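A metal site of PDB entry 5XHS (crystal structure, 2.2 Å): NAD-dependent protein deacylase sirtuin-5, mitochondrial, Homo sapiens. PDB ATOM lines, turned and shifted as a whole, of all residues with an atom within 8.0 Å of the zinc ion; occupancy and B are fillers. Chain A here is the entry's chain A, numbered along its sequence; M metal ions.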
ATOM      1  N   ARG A 151      11.886  10.572  17.510  1.00  0.00           N
ATOM      2  CA  ARG A 151      11.390  10.567  16.147  1.00  0.00           C
ATOM      3  C   ARG A 151      12.338   9.805  15.244  1.00  0.00           C
ATOM      4  O   ARG A 151      13.551  10.048  15.261  1.00  0.00           O
ATOM      5  CB  ARG A 151      11.233  11.990  15.618  1.00  0.00           C
ATOM      6  CG  ARG A 151      10.549  12.114  14.251  1.00  0.00           C
ATOM      7  CD  ARG A 151      10.077  13.534  14.062  1.00  0.00           C
ATOM      8  NE  ARG A 151      11.090  14.479  13.575  1.00  0.00           N
ATOM      9  CZ  ARG A 151      11.421  15.649  14.145  1.00  0.00           C
ATOM     10  NH1 ARG A 151      10.890  16.051  15.292  1.00  0.00           N
ATOM     11  NH2 ARG A 151      12.302  16.437  13.560  1.00  0.00           N
ATOM     12  N   CYS A 152      11.794   8.887  14.461  1.00  0.00           N
ATOM     13  CA  CYS A 152      12.623   8.103  13.549  1.00  0.00           C
ATOM     14  C   CYS A 152      13.022   8.939  12.336  1.00  0.00           C
ATOM     15  O   CYS A 152      12.173   9.500  11.654  1.00  0.00           O
ATOM     16  CB  CYS A 152      11.895   6.853  13.070  1.00  0.00           C
ATOM     17  SG  CYS A 152      12.989   5.876  12.044  1.00  0.00           S
ATOM     18  N   THR A 153      14.322   9.027  12.069  1.00  0.00           N
ATOM     19  CA  THR A 153      14.775   9.813  10.934  1.00  0.00           C
ATOM     20  C   THR A 153      14.504   9.108   9.616  1.00  0.00           C
ATOM     21  O   THR A 153      14.757   9.714   8.573  1.00  0.00           O
ATOM     22  CB  THR A 153      16.265  10.141  11.054  1.00  0.00           C
ATOM     23  OG1 THR A 153      17.044   8.960  10.865  1.00  0.00           O
ATOM     24  CG2 THR A 153      16.598  10.727  12.425  1.00  0.00           C
ATOM     25  N   SER A 154      14.008   7.860   9.637  1.00  0.00           N
ATOM     26  CA  SER A 154      13.585   7.159   8.424  1.00  0.00           C
ATOM     27  C   SER A 154      12.072   7.165   8.251  1.00  0.00           C
ATOM     28  O   SER A 154      11.582   7.675   7.242  1.00  0.00           O
ATOM     29  CB  SER A 154      14.097   5.712   8.434  1.00  0.00           C
ATOM     30  OG  SER A 154      15.488   5.710   8.616  1.00  0.00           O
ATOM     31  N   CYS A 155      11.311   6.638   9.198  1.00  0.00           N
ATOM     32  CA  CYS A 155       9.869   6.539   8.976  1.00  0.00           C
ATOM     33  C   CYS A 155       9.080   7.705   9.575  1.00  0.00           C
ATOM     34  O   CYS A 155       7.861   7.798   9.334  1.00  0.00           O
ATOM     35  CB  CYS A 155       9.333   5.202   9.538  1.00  0.00           C
ATOM     36  SG  CYS A 155       9.306   5.014  11.312  1.00  0.00           S
ATOM     37  N   GLY A 156       9.729   8.563  10.357  1.00  0.00           N
ATOM     38  CA  GLY A 156       9.079   9.702  10.983  1.00  0.00           C
ATOM     39  C   GLY A 156       8.153   9.410  12.142  1.00  0.00           C
ATOM     40  O   GLY A 156       7.479  10.321  12.635  1.00  0.00           O
ATOM     41  N   VAL A 157       8.094   8.164  12.614  1.00  0.00           N
ATOM     42  CA  VAL A 157       7.184   7.864  13.718  1.00  0.00           C
ATOM     43  C   VAL A 157       7.682   8.562  14.983  1.00  0.00           C
ATOM     44  O   VAL A 157       8.890   8.603  15.260  1.00  0.00           O
ATOM     45  CB  VAL A 157       7.058   6.342  13.908  1.00  0.00           C
ATOM     46  CG1 VAL A 157       6.290   5.987  15.130  1.00  0.00           C
ATOM     47  CG2 VAL A 157       6.345   5.728  12.729  1.00  0.00           C
ATOM     48  N   VAL A 158       6.759   9.138  15.737  1.00  0.00           N
ATOM     49  CA  VAL A 158       7.058   9.779  17.010  1.00  0.00           C
ATOM     50  C   VAL A 158       6.594   8.855  18.129  1.00  0.00           C
ATOM     51  O   VAL A 158       5.468   8.347  18.097  1.00  0.00           O
ATOM     52  CB  VAL A 158       6.389  11.157  17.101  1.00  0.00           C
ATOM     53  CG1 VAL A 158       6.721  11.862  18.411  1.00  0.00           C
ATOM     54  CG2 VAL A 158       6.810  12.016  15.944  1.00  0.00           C
ATOM     55  N   ARG A 192      17.521   3.142  18.222  1.00  0.00           N
ATOM     56  CA  ARG A 192      16.998   2.727  16.940  1.00  0.00           C
ATOM     57  C   ARG A 192      15.488   2.626  16.999  1.00  0.00           C
ATOM     58  O   ARG A 192      14.915   2.332  18.054  1.00  0.00           O
ATOM     59  CB  ARG A 192      17.560   1.371  16.511  1.00  0.00           C
ATOM     60  CG  ARG A 192      19.076   1.292  16.494  1.00  0.00           C
ATOM     61  CD  ARG A 192      19.738   2.371  15.625  1.00  0.00           C
ATOM     62  NE  ARG A 192      19.425   2.250  14.199  1.00  0.00           N
ATOM     63  CZ  ARG A 192      20.173   2.733  13.207  1.00  0.00           C
ATOM     64  NH1 ARG A 192      21.311   3.374  13.449  1.00  0.00           N
ATOM     65  NH2 ARG A 192      19.785   2.569  11.945  1.00  0.00           N
ATOM     66  N   CYS A 193      14.879   2.829  15.844  1.00  0.00           N
ATOM     67  CA  CYS A 193      13.438   2.710  15.720  1.00  0.00           C
ATOM     68  C   CYS A 193      13.030   1.271  15.966  1.00  0.00           C
ATOM     69  O   CYS A 193      13.630   0.342  15.418  1.00  0.00           O
ATOM     70  CB  CYS A 193      12.980   3.154  14.328  1.00  0.00           C
ATOM     71  SG  CYS A 193      11.194   3.165  14.168  1.00  0.00           S
ATOM     72  N   GLU A 194      11.991   1.100  16.785  1.00  0.00           N
ATOM     73  CA  GLU A 194      11.436  -0.203  17.110  1.00  0.00           C
ATOM     74  C   GLU A 194      10.154  -0.508  16.312  1.00  0.00           C
ATOM     75  O   GLU A 194       9.512  -1.527  16.555  1.00  0.00           O
ATOM     76  CB  GLU A 194      11.208  -0.284  18.616  1.00  0.00           C
ATOM     77  CG  GLU A 194      12.443  -0.810  19.335  1.00  0.00           C
ATOM     78  CD  GLU A 194      12.441  -0.577  20.824  1.00  0.00           C
ATOM     79  OE1 GLU A 194      11.427  -0.895  21.474  1.00  0.00           O
ATOM     80  OE2 GLU A 194      13.479  -0.069  21.335  1.00  0.00           O
ATOM     81  N   GLU A 195       9.770   0.339  15.371  1.00  0.00           N
ATOM     82  CA  GLU A 195       8.670  -0.007  14.491  1.00  0.00           C
ATOM     83  C   GLU A 195       9.052  -1.238  13.670  1.00  0.00           C
ATOM     84  O   GLU A 195      10.168  -1.328  13.136  1.00  0.00           O
ATOM     85  CB  GLU A 195       8.313   1.183  13.580  1.00  0.00           C
ATOM     86  CG  GLU A 195       7.652   2.325  14.319  1.00  0.00           C
ATOM     87  CD  GLU A 195       6.275   1.940  14.810  1.00  0.00           C
ATOM     88  OE1 GLU A 195       5.373   1.771  13.960  1.00  0.00           O
ATOM     89  OE2 GLU A 195       6.090   1.767  16.039  1.00  0.00           O
ATOM     90  N   ALA A 196       8.136  -2.202  13.601  1.00  0.00           N
ATOM     91  CA  ALA A 196       8.365  -3.395  12.787  1.00  0.00           C
ATOM     92  C   ALA A 196       8.797  -3.011  11.380  1.00  0.00           C
ATOM     93  O   ALA A 196       8.096  -2.300  10.655  1.00  0.00           O
ATOM     94  CB  ALA A 196       7.099  -4.255  12.736  1.00  0.00           C
ATOM     95  N   GLY A 197       9.971  -3.492  10.984  1.00  0.00           N
ATOM     96  CA  GLY A 197      10.456  -3.275   9.644  1.00  0.00           C
ATOM     97  C   GLY A 197      11.062  -1.924   9.382  1.00  0.00           C
ATOM     98  O   GLY A 197      11.138  -1.538   8.216  1.00  0.00           O
ATOM     99  N   CYS A 198      11.502  -1.194  10.405  1.00  0.00           N
ATOM    100  CA  CYS A 198      12.160   0.084  10.167  1.00  0.00           C
ATOM    101  C   CYS A 198      13.601   0.068  10.665  1.00  0.00           C
ATOM    102  O   CYS A 198      14.520   0.068   9.837  1.00  0.00           O
ATOM    103  CB  CYS A 198      11.379   1.246  10.790  1.00  0.00           C
ATOM    104  SG  CYS A 198      12.220   2.772  10.397  1.00  0.00           S
ATOM    105  N   GLY A 199      13.840   0.076  11.978  1.00  0.00           N
ATOM    106  CA  GLY A 199      15.207   0.089  12.492  1.00  0.00           C
ATOM    107  C   GLY A 199      16.081   1.295  12.152  1.00  0.00           C
ATOM    108  O   GLY A 199      17.298   1.203  12.306  1.00  0.00           O
ATOM    109  N   GLY A 200      15.518   2.416  11.725  1.00  0.00           N
ATOM    110  CA  GLY A 200      16.324   3.590  11.469  1.00  0.00           C
ATOM    111  C   GLY A 200      16.853   4.275  12.739  1.00  0.00           C
ATOM    112  O   GLY A 200      16.495   3.952  13.871  1.00  0.00           O
ATOM    113  N   LEU A 201      17.694   5.285  12.526  1.00  0.00           N
ATOM    114  CA  LEU A 201      18.297   6.033  13.621  1.00  0.00           C
ATOM    115  C   LEU A 201      17.297   7.025  14.217  1.00  0.00           C
ATOM    116  O   LEU A 201      16.796   7.903  13.503  1.00  0.00           O
ATOM    117  CB  LEU A 201      19.545   6.764  13.128  1.00  0.00           C
ATOM    118  CG  LEU A 201      20.205   7.676  14.162  1.00  0.00           C
ATOM    119  CD1 LEU A 201      20.877   6.848  15.247  1.00  0.00           C
ATOM    120  CD2 LEU A 201      21.208   8.586  13.500  1.00  0.00           C
ATOM    121  N   LEU A 202      17.012   6.902  15.514  1.00  0.00           N
ATOM    122  CA  LEU A 202      16.183   7.866  16.212  1.00  0.00           C
ATOM    123  C   LEU A 202      16.942   9.161  16.464  1.00  0.00           C
ATOM    124  O   LEU A 202      18.170   9.188  16.645  1.00  0.00           O
ATOM    125  CB  LEU A 202      15.686   7.326  17.549  1.00  0.00           C
ATOM    126  CG  LEU A 202      14.890   6.028  17.466  1.00  0.00           C
ATOM    127  CD1 LEU A 202      14.471   5.586  18.869  1.00  0.00           C
ATOM    128  CD2 LEU A 202      13.652   6.211  16.569  1.00  0.00           C
HETATM  129 ZN    ZN M   1      11.346   4.178  12.001  1.00  0.00          ZN
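The side-chain sulfur of Cys 198 lies close to the backbone NH of Gly 200, 3.6 Å away. N of Val 157 sits close to SG of Cys 155, at 3.6 Å. N of Ser 154 sits close to SG of Cys 152 (3.3 Å). The backbone NH (N) of Cys 152 lies within hydrogen-bond range of the backbone carbonyl oxygen (O) of Val 157 (3.0 Å). O of Gly 200 is in hydrogen-bond range of N of Cys 193, at 2.8 Å. The backbone NH (N) of Glu 195 lies close to the side-chain sulfur (SG) of Cys 193, 3.4 Å away. The backbone carbonyl oxygen (O) of Cys 193 sits close to the backbone NH (N) of Gly 199 (3.5 Å).
The nearest printed residue that does not touch the zinc ion is Gly 200 (4.5 Å).
The zinc ion is bound by the side-chain sulfur (SG) of Cys 198 (2.3 Å), the side-chain sulfur (SG) of Cys 155 (2.3 Å), the side-chain sulfur (SG) of Cys 152 (2.4 Å) and the side-chain sulfur (SG) of Cys 193 (2.4 Å).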
